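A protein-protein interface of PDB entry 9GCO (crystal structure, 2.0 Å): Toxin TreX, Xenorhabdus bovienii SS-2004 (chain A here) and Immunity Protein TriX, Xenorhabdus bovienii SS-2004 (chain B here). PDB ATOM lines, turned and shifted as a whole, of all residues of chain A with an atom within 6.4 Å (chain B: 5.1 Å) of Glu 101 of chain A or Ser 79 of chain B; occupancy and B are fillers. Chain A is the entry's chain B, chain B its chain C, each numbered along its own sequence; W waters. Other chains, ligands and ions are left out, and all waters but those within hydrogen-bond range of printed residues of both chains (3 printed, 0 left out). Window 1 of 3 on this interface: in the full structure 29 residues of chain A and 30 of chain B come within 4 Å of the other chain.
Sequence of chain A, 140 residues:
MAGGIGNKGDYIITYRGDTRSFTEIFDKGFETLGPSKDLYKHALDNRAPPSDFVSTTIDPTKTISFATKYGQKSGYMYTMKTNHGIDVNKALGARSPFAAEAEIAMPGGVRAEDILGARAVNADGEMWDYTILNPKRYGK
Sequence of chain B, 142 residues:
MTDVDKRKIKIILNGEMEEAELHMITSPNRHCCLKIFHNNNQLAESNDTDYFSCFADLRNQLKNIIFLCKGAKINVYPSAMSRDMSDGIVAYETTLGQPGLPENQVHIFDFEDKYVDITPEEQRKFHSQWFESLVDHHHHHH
Water W3 lies within hydrogen-bond range of OE1 of Glu 101 of chain A, N of Met 81 of chain B, OE1 of Glu 103 of chain A and N of Ala 80 of chain B. Water W1 lies within hydrogen-bond range of the guanidinium group of Arg 83 of chain B (2.8 Å), the backbone carbonyl oxygen of Pro 78 of chain B (3.0 Å) and the side-chain amide oxygen of Asn 46 of chain A (3.3 Å). Water W2 lies within hydrogen-bond range of the backbone carbonyl oxygen (O) of Ala 43 of chain A (2.8 Å) and the backbone NH (N) of Ala 80 of chain B (3.0 Å).
Of the 9 printed residues of chain B, 6 touch a printed residue of chain A. Printed residues of chain B that touch a printed residue of chain A: Ser 79, Ala 80, Met 81, Ser 82, Arg 83 and Tyr 92. Hydrophobic or aromatic side chains of chain B that line the printed part of chain A: Ala 80, Met 81 and Tyr 92. Among the printed residues, 14 pairs touch across the chains. Among the printed residues, no Asp or Glu carboxylate lies within 4 Å of a Lys or Arg side-chain nitrogen of the other chain.
The backbone NH of Tyr 92 of chain B is in hydrogen-bond range of the backbone carbonyl oxygen of Tyr 77 of chain B. OG of Ser 79 of chain B is in hydrogen-bond range of N of Ser 82 of chain B (2.9 Å). OG of Ser 79 of chain B lies close to N of Met 81 of chain B, at 3.3 Å. The backbone carbonyl oxygen of Thr 56 of chain A is in hydrogen-bond range of the backbone NH of Ile 104 of chain A. The side-chain hydroxyl of Thr 57 of chain A sits at hydrogen-bond distance from the backbone carbonyl oxygen of Glu 101 of chain A, at 2.7 Å. The backbone carbonyl oxygen of Ala 102 of chain A sits at hydrogen-bond distance from the side-chain hydroxyl of Thr 57 of chain A, at 3.3 Å.
OG of Ser 79 of chain B is in hydrogen-bond range of OE2 of Glu 101 of chain A. The side-chain amide nitrogen of Asn 46 of chain A lies within hydrogen-bond range of the backbone carbonyl oxygen of Ala 80 of chain B (3.4 Å). The side-chain amide oxygen of Asn 46 of chain A sits at hydrogen-bond distance from the guanidinium group of Arg 83 of chain B, at 3.1 Å. OE2 of Glu 101 of chain A lies within hydrogen-bond range of OH of Tyr 92 of chain B, at 2.6 Å.
Of chain B, only Ser 79 (2.6 Å), Met 81 (3.5 Å) and Tyr 92 (2.6 Å) come within 4 Å of Glu 101 of chain A. Of chain A, only Phe 98 (3.4 Å) and Glu 101 (2.6 Å) come within 4 Å of Ser 79 of chain B. Of the printed residues of chain B, His 42 of chain A touches Ala 80. Of the printed residues of chain B, Phe 66 of chain A touches Met 81, Ser 82 and Tyr 92. Of the printed residues of chain B, Phe 98 of chain A touches Ser 79 and Tyr 92. Ile 58 of chain A touches none of the printed residues of chain B. Tyr 77 of chain B touches none of the printed residues of chain A. The nearest residue of chain B that does not touch Glu 101 of chain A is Ser 82 of chain B (4.4 Å). The nearest residue of chain A that does not touch Ser 79 of chain B is Asn 46 of chain A (4.5 Å).
Among the printed residues, pairs that only touch across the chains: His 42 of chain A with Ala 80 of chain B, Thr 56 of chain A with Met 81 of chain B, Thr 57 of chain A with Met 81 of chain B, Phe 66 of chain A with Met 81 of chain B, Phe 66 of chain A with Ser 82 of chain B, Phe 66 of chain A with Tyr 92 of chain B, Phe 98 of chain A with Ser 79 of chain B, Phe 98 of chain A with Tyr 92 of chain B, Glu 101 of chain A with Met 81 of chain B and Glu 103 of chain A with Met 81 of chain B.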
ATOM      1  N   HIS A  42     -15.495 -23.610  10.460  1.00  0.00           N
ATOM      2  CA  HIS A  42     -15.985 -24.431  11.565  1.00  0.00           C
ATOM      3  C   HIS A  42     -16.371 -23.567  12.756  1.00  0.00           C
ATOM      4  O   HIS A  42     -17.395 -23.815  13.405  1.00  0.00           O
ATOM      5  CB  HIS A  42     -14.924 -25.459  11.966  1.00  0.00           C
ATOM      6  CG  HIS A  42     -15.184 -26.115  13.283  1.00  0.00           C
ATOM      7  ND1 HIS A  42     -15.925 -27.274  13.409  1.00  0.00           N
ATOM      8  CD2 HIS A  42     -14.809 -25.766  14.536  1.00  0.00           C
ATOM      9  CE1 HIS A  42     -16.000 -27.600  14.688  1.00  0.00           C
ATOM     10  NE2 HIS A  42     -15.320 -26.711  15.390  1.00  0.00           N
ATOM     11  N   ALA A  43     -15.548 -22.552  13.062  1.00  0.00           N
ATOM     12  CA  ALA A  43     -15.797 -21.689  14.211  1.00  0.00           C
ATOM     13  C   ALA A  43     -16.993 -20.769  13.979  1.00  0.00           C
ATOM     14  O   ALA A  43     -17.824 -20.598  14.874  1.00  0.00           O
ATOM     15  CB  ALA A  43     -14.540 -20.860  14.498  1.00  0.00           C
ATOM     16  N   ASN A  46     -20.398 -24.428  12.183  1.00  0.00           N
ATOM     17  CA  ASN A  46     -19.918 -25.751  11.821  1.00  0.00           C
ATOM     18  C   ASN A  46     -20.991 -26.582  11.130  1.00  0.00           C
ATOM     19  O   ASN A  46     -20.737 -27.742  10.802  1.00  0.00           O
ATOM     20  CB  ASN A  46     -19.366 -26.500  13.051  1.00  0.00           C
ATOM     21  CG  ASN A  46     -20.428 -26.811  14.093  1.00  0.00           C
ATOM     22  OD1 ASN A  46     -21.397 -26.074  14.263  1.00  0.00           O
ATOM     23  ND2 ASN A  46     -20.216 -27.916  14.831  1.00  0.00           N
ATOM     24  N   THR A  56     -14.056 -31.247  21.153  1.00  0.00           N
ATOM     25  CA  THR A  56     -13.740 -31.733  22.492  1.00  0.00           C
ATOM     26  C   THR A  56     -13.145 -30.562  23.270  1.00  0.00           C
ATOM     27  O   THR A  56     -12.839 -29.509  22.698  1.00  0.00           O
ATOM     28  CB  THR A  56     -12.773 -32.925  22.485  1.00  0.00           C
ATOM     29  OG1 THR A  56     -11.436 -32.482  22.194  1.00  0.00           O
ATOM     30  CG2 THR A  56     -13.189 -33.978  21.439  1.00  0.00           C
ATOM     31  N   THR A  57     -12.964 -30.735  24.584  1.00  0.00           N
ATOM     32  CA  THR A  57     -12.425 -29.650  25.401  1.00  0.00           C
ATOM     33  C   THR A  57     -11.349 -30.212  26.305  1.00  0.00           C
ATOM     34  O   THR A  57     -11.374 -31.394  26.659  1.00  0.00           O
ATOM     35  CB  THR A  57     -13.521 -28.951  26.215  1.00  0.00           C
ATOM     36  OG1 THR A  57     -12.964 -27.937  27.064  1.00  0.00           O
ATOM     37  CG2 THR A  57     -14.255 -29.946  27.113  1.00  0.00           C
ATOM     38  N   ILE A  58     -10.383 -29.359  26.662  1.00  0.00           N
ATOM     39  CA  ILE A  58      -9.410 -29.767  27.672  1.00  0.00           C
ATOM     40  C   ILE A  58      -9.918 -29.490  29.072  1.00  0.00           C
ATOM     41  O   ILE A  58      -9.234 -29.814  30.047  1.00  0.00           O
ATOM     42  CB  ILE A  58      -8.043 -29.074  27.521  1.00  0.00           C
ATOM     43  CG1 ILE A  58      -8.181 -27.532  27.572  1.00  0.00           C
ATOM     44  CG2 ILE A  58      -7.380 -29.463  26.203  1.00  0.00           C
ATOM     45  CD1 ILE A  58      -6.805 -26.830  27.725  1.00  0.00           C
ATOM     46  N   ASP A  59     -11.099 -28.851  29.210  1.00  0.00           N
ATOM     47  CA  ASP A  59     -11.636 -28.493  30.520  1.00  0.00           C
ATOM     48  C   ASP A  59     -12.882 -29.313  30.776  1.00  0.00           C
ATOM     49  O   ASP A  59     -13.952 -29.012  30.205  1.00  0.00           O
ATOM     50  CB  ASP A  59     -11.982 -26.997  30.561  1.00  0.00           C
ATOM     51  CG  ASP A  59     -12.433 -26.531  31.950  1.00  0.00           C
ATOM     52  OD1 ASP A  59     -12.677 -27.367  32.862  1.00  0.00           O
ATOM     53  OD2 ASP A  59     -12.549 -25.300  32.131  1.00  0.00           O
ATOM     54  N   LYS A  62     -16.464 -27.865  31.379  1.00  0.00           N
ATOM     55  CA  LYS A  62     -17.200 -27.265  30.278  1.00  0.00           C
ATOM     56  C   LYS A  62     -18.152 -28.241  29.600  1.00  0.00           C
ATOM     57  O   LYS A  62     -18.978 -27.802  28.801  1.00  0.00           O
ATOM     58  CB  LYS A  62     -16.212 -26.701  29.256  1.00  0.00           C
ATOM     59  CG  LYS A  62     -15.272 -25.623  29.861  1.00  0.00           C
ATOM     60  CD  LYS A  62     -15.946 -24.258  29.888  1.00  0.00           C
ATOM     61  CE  LYS A  62     -15.474 -23.377  31.051  1.00  0.00           C
ATOM     62  NZ  LYS A  62     -14.039 -22.976  30.916  1.00  0.00           N
ATOM     63  N   PHE A  66     -23.555 -28.918  28.563  1.00  0.00           N
ATOM     64  CA  PHE A  66     -23.946 -29.479  27.277  1.00  0.00           C
ATOM     65  C   PHE A  66     -24.519 -30.876  27.453  1.00  0.00           C
ATOM     66  O   PHE A  66     -25.569 -31.209  26.893  1.00  0.00           O
ATOM     67  CB  PHE A  66     -22.733 -29.502  26.347  1.00  0.00           C
ATOM     68  CG  PHE A  66     -22.202 -28.132  26.030  1.00  0.00           C
ATOM     69  CD1 PHE A  66     -23.053 -27.039  25.959  1.00  0.00           C
ATOM     70  CD2 PHE A  66     -20.847 -27.936  25.835  1.00  0.00           C
ATOM     71  CE1 PHE A  66     -22.567 -25.766  25.668  1.00  0.00           C
ATOM     72  CE2 PHE A  66     -20.349 -26.657  25.563  1.00  0.00           C
ATOM     73  CZ  PHE A  66     -21.218 -25.577  25.469  1.00  0.00           C
ATOM     74  N   ASN A  89      -8.139 -22.101  19.827  1.00  0.00           N
ATOM     75  CA  ASN A  89      -7.642 -20.785  20.245  1.00  0.00           C
ATOM     76  C   ASN A  89      -6.258 -20.531  19.684  1.00  0.00           C
ATOM     77  O   ASN A  89      -5.924 -19.400  19.301  1.00  0.00           O
ATOM     78  CB  ASN A  89      -7.573 -20.683  21.775  1.00  0.00           C
ATOM     79  CG  ASN A  89      -8.932 -20.758  22.408  1.00  0.00           C
ATOM     80  OD1 ASN A  89      -9.938 -20.653  21.721  1.00  0.00           O
ATOM     81  ND2 ASN A  89      -8.969 -20.947  23.722  1.00  0.00           N
ATOM     82  N   PHE A  98     -15.369 -18.356  20.969  1.00  0.00           N
ATOM     83  CA  PHE A  98     -15.786 -18.894  22.252  1.00  0.00           C
ATOM     84  C   PHE A  98     -14.538 -19.449  22.927  1.00  0.00           C
ATOM     85  O   PHE A  98     -14.453 -20.624  23.296  1.00  0.00           O
ATOM     86  CB  PHE A  98     -16.874 -19.955  22.090  1.00  0.00           C
ATOM     87  CG  PHE A  98     -18.062 -19.480  21.314  1.00  0.00           C
ATOM     88  CD1 PHE A  98     -19.082 -18.772  21.950  1.00  0.00           C
ATOM     89  CD2 PHE A  98     -18.174 -19.738  19.952  1.00  0.00           C
ATOM     90  CE1 PHE A  98     -20.181 -18.313  21.244  1.00  0.00           C
ATOM     91  CE2 PHE A  98     -19.293 -19.253  19.214  1.00  0.00           C
ATOM     92  CZ  PHE A  98     -20.286 -18.547  19.869  1.00  0.00           C
ATOM     93  N   ALA A  99     -13.550 -18.565  23.110  1.00  0.00           N
ATOM     94  CA  ALA A  99     -12.256 -18.957  23.655  1.00  0.00           C
ATOM     95  C   ALA A  99     -12.368 -19.763  24.945  1.00  0.00           C
ATOM     96  O   ALA A  99     -11.590 -20.695  25.157  1.00  0.00           O
ATOM     97  CB  ALA A  99     -11.400 -17.718  23.916  1.00  0.00           C
ATOM     98  N   ALA A 100     -13.325 -19.437  25.819  1.00  0.00           N
ATOM     99  CA  ALA A 100     -13.349 -20.101  27.118  1.00  0.00           C
ATOM    100  C   ALA A 100     -13.775 -21.567  27.042  1.00  0.00           C
ATOM    101  O   ALA A 100     -13.706 -22.275  28.062  1.00  0.00           O
ATOM    102  CB  ALA A 100     -14.304 -19.400  28.093  1.00  0.00           C
ATOM    103  N   GLU A 101     -14.272 -22.024  25.899  1.00  0.00           N
ATOM    104  CA  GLU A 101     -14.565 -23.450  25.763  1.00  0.00           C
ATOM    105  C   GLU A 101     -13.295 -24.306  25.748  1.00  0.00           C
ATOM    106  O   GLU A 101     -13.375 -25.499  26.053  1.00  0.00           O
ATOM    107  CB  GLU A 101     -15.391 -23.697  24.501  1.00  0.00           C
ATOM    108  CG  GLU A 101     -16.798 -23.059  24.542  1.00  0.00           C
ATOM    109  CD  GLU A 101     -17.539 -23.244  23.245  1.00  0.00           C
ATOM    110  OE1 GLU A 101     -16.864 -23.442  22.191  1.00  0.00           O
ATOM    111  OE2 GLU A 101     -18.785 -23.189  23.277  1.00  0.00           O
ATOM    112  N   ALA A 102     -12.135 -23.717  25.462  1.00  0.00           N
ATOM    113  CA  ALA A 102     -10.868 -24.447  25.382  1.00  0.00           C
ATOM    114  C   ALA A 102     -11.007 -25.677  24.476  1.00  0.00           C
ATOM    115  O   ALA A 102     -10.803 -26.813  24.896  1.00  0.00           O
ATOM    116  CB  ALA A 102     -10.391 -24.859  26.774  1.00  0.00           C
ATOM    117  N   GLU A 103     -11.425 -25.413  23.243  1.00  0.00           N
ATOM    118  CA  GLU A 103     -11.834 -26.434  22.287  1.00  0.00           C
ATOM    119  C   GLU A 103     -10.630 -27.039  21.575  1.00  0.00           C
ATOM    120  O   GLU A 103      -9.737 -26.315  21.097  1.00  0.00           O
ATOM    121  CB  GLU A 103     -12.789 -25.821  21.257  1.00  0.00           C
ATOM    122  CG  GLU A 103     -13.450 -26.820  20.285  1.00  0.00           C
ATOM    123  CD  GLU A 103     -14.242 -26.160  19.127  1.00  0.00           C
ATOM    124  OE1 GLU A 103     -14.403 -24.924  19.118  1.00  0.00           O
ATOM    125  OE2 GLU A 103     -14.681 -26.893  18.189  1.00  0.00           O
ATOM    126  N   ILE A 104     -10.616 -28.368  21.503  1.00  0.00           N
ATOM    127  CA  ILE A 104      -9.686 -29.126  20.675  1.00  0.00           C
ATOM    128  C   ILE A 104     -10.526 -29.752  19.560  1.00  0.00           C
ATOM    129  O   ILE A 104     -11.287 -30.693  19.823  1.00  0.00           O
ATOM    130  CB  ILE A 104      -8.943 -30.203  21.474  1.00  0.00           C
ATOM    131  CG1 ILE A 104      -8.188 -29.594  22.663  1.00  0.00           C
ATOM    132  CG2 ILE A 104      -7.944 -30.921  20.559  1.00  0.00           C
ATOM    133  CD1 ILE A 104      -6.995 -28.699  22.280  1.00  0.00           C
ATOM    134  N   TYR B  77     -26.933 -17.797  19.064  1.00  0.00           N
ATOM    135  CA  TYR B  77     -26.463 -18.795  18.105  1.00  0.00           C
ATOM    136  C   TYR B  77     -25.639 -19.823  18.857  1.00  0.00           C
ATOM    137  O   TYR B  77     -24.957 -19.467  19.818  1.00  0.00           O
ATOM    138  CB  TYR B  77     -25.612 -18.139  16.997  1.00  0.00           C
ATOM    139  CG  TYR B  77     -25.791 -18.728  15.611  1.00  0.00           C
ATOM    140  CD1 TYR B  77     -26.904 -18.404  14.850  1.00  0.00           C
ATOM    141  CD2 TYR B  77     -24.828 -19.596  15.055  1.00  0.00           C
ATOM    142  CE1 TYR B  77     -27.089 -18.939  13.556  1.00  0.00           C
ATOM    143  CE2 TYR B  77     -25.003 -20.141  13.767  1.00  0.00           C
ATOM    144  CZ  TYR B  77     -26.129 -19.798  13.028  1.00  0.00           C
ATOM    145  OH  TYR B  77     -26.315 -20.318  11.767  1.00  0.00           O
ATOM    146  N   PRO B  78     -25.668 -21.090  18.453  1.00  0.00           N
ATOM    147  CA  PRO B  78     -24.811 -22.071  19.118  1.00  0.00           C
ATOM    148  C   PRO B  78     -23.381 -21.917  18.643  1.00  0.00           C
ATOM    149  O   PRO B  78     -23.119 -21.415  17.545  1.00  0.00           O
ATOM    150  CB  PRO B  78     -25.398 -23.417  18.692  1.00  0.00           C
ATOM    151  CG  PRO B  78     -26.072 -23.137  17.405  1.00  0.00           C
ATOM    152  CD  PRO B  78     -26.539 -21.724  17.439  1.00  0.00           C
ATOM    153  N   SER B  79     -22.462 -22.291  19.525  1.00  0.00           N
ATOM    154  CA  SER B  79     -21.072 -22.509  19.145  1.00  0.00           C
ATOM    155  C   SER B  79     -20.961 -23.863  18.462  1.00  0.00           C
ATOM    156  O   SER B  79     -21.882 -24.691  18.523  1.00  0.00           O
ATOM    157  CB  SER B  79     -20.147 -22.440  20.361  1.00  0.00           C
ATOM    158  OG  SER B  79     -20.295 -23.573  21.229  1.00  0.00           O
ATOM    159  N   ALA B  80     -19.837 -24.075  17.773  1.00  0.00           N
ATOM    160  CA  ALA B  80     -19.560 -25.405  17.251  1.00  0.00           C
ATOM    161  C   ALA B  80     -19.689 -26.444  18.356  1.00  0.00           C
ATOM    162  O   ALA B  80     -20.333 -27.488  18.198  1.00  0.00           O
ATOM    163  CB  ALA B  80     -18.151 -25.471  16.630  1.00  0.00           C
ATOM    164  N   MET B  81     -19.080 -26.159  19.496  1.00  0.00           N
ATOM    165  CA  MET B  81     -19.061 -27.134  20.569  1.00  0.00           C
ATOM    166  C   MET B  81     -20.451 -27.352  21.153  1.00  0.00           C
ATOM    167  O   MET B  81     -20.841 -28.493  21.427  1.00  0.00           O
ATOM    168  CB  MET B  81     -18.092 -26.676  21.655  1.00  0.00           C
ATOM    169  CG  MET B  81     -18.073 -27.653  22.821  1.00  0.00           C
ATOM    170  SD  MET B  81     -16.850 -27.278  24.053  1.00  0.00           S
ATOM    171  CE  MET B  81     -15.361 -27.419  23.070  1.00  0.00           C
ATOM    172  N   SER B  82     -21.214 -26.271  21.348  1.00  0.00           N
ATOM    173  CA  SER B  82     -22.533 -26.400  21.979  1.00  0.00           C
ATOM    174  C   SER B  82     -23.511 -27.084  21.029  1.00  0.00           C
ATOM    175  O   SER B  82     -24.345 -27.886  21.459  1.00  0.00           O
ATOM    176  CB  SER B  82     -23.054 -25.023  22.453  1.00  0.00           C
ATOM    177  OG  SER B  82     -23.661 -24.233  21.444  1.00  0.00           O
ATOM    178  N   ARG B  83     -23.405 -26.801  19.733  1.00  0.00           N
ATOM    179  CA  ARG B  83     -24.238 -27.486  18.752  1.00  0.00           C
ATOM    180  C   ARG B  83     -23.939 -28.973  18.777  1.00  0.00           C
ATOM    181  O   ARG B  83     -24.844 -29.805  18.877  1.00  0.00           O
ATOM    182  CB  ARG B  83     -23.990 -26.907  17.353  1.00  0.00           C
ATOM    183  CG  ARG B  83     -24.944 -27.442  16.260  1.00  0.00           C
ATOM    184  CD  ARG B  83     -24.564 -26.995  14.804  1.00  0.00           C
ATOM    185  NE  ARG B  83     -24.486 -25.551  14.578  1.00  0.00           N
ATOM    186  CZ  ARG B  83     -25.485 -24.776  14.158  1.00  0.00           C
ATOM    187  NH1 ARG B  83     -26.715 -25.243  13.983  1.00  0.00           N
ATOM    188  NH2 ARG B  83     -25.240 -23.498  13.907  1.00  0.00           N
ATOM    189  N   ASP B  84     -22.649 -29.309  18.780  1.00  0.00           N
ATOM    190  CA  ASP B  84     -22.197 -30.692  18.724  1.00  0.00           C
ATOM    191  C   ASP B  84     -22.522 -31.432  20.018  1.00  0.00           C
ATOM    192  O   ASP B  84     -23.186 -32.477  19.994  1.00  0.00           O
ATOM    193  CB  ASP B  84     -20.688 -30.688  18.440  1.00  0.00           C
ATOM    194  CG  ASP B  84     -20.198 -31.968  17.836  1.00  0.00           C
ATOM    195  OD1 ASP B  84     -21.020 -32.905  17.718  1.00  0.00           O
ATOM    196  OD2 ASP B  84     -18.983 -32.061  17.523  1.00  0.00           O
ATOM    197  N   TYR B  92     -25.644 -19.535  22.682  1.00  0.00           N
ATOM    198  CA  TYR B  92     -25.113 -18.360  23.375  1.00  0.00           C
ATOM    199  C   TYR B  92     -25.831 -17.083  22.978  1.00  0.00           C
ATOM    200  O   TYR B  92     -26.176 -16.905  21.797  1.00  0.00           O
ATOM    201  CB  TYR B  92     -23.642 -18.148  23.041  1.00  0.00           C
ATOM    202  CG  TYR B  92     -22.681 -19.153  23.617  1.00  0.00           C
ATOM    203  CD1 TYR B  92     -22.535 -20.409  23.047  1.00  0.00           C
ATOM    204  CD2 TYR B  92     -21.914 -18.836  24.695  1.00  0.00           C
ATOM    205  CE1 TYR B  92     -21.628 -21.328  23.567  1.00  0.00           C
ATOM    206  CE2 TYR B  92     -20.984 -19.749  25.238  1.00  0.00           C
ATOM    207  CZ  TYR B  92     -20.867 -20.991  24.666  1.00  0.00           C
ATOM    208  OH  TYR B  92     -19.967 -21.876  25.167  1.00  0.00           O
HETATM  209  O   HOH W   1     -22.758 -23.188  15.111  1.00  0.00           O
HETATM  210  O   HOH W   2     -17.799 -21.891  17.360  1.00  0.00           O
HETATM  211  O   HOH W   3     -17.104 -24.117  19.579  1.00  0.00           O
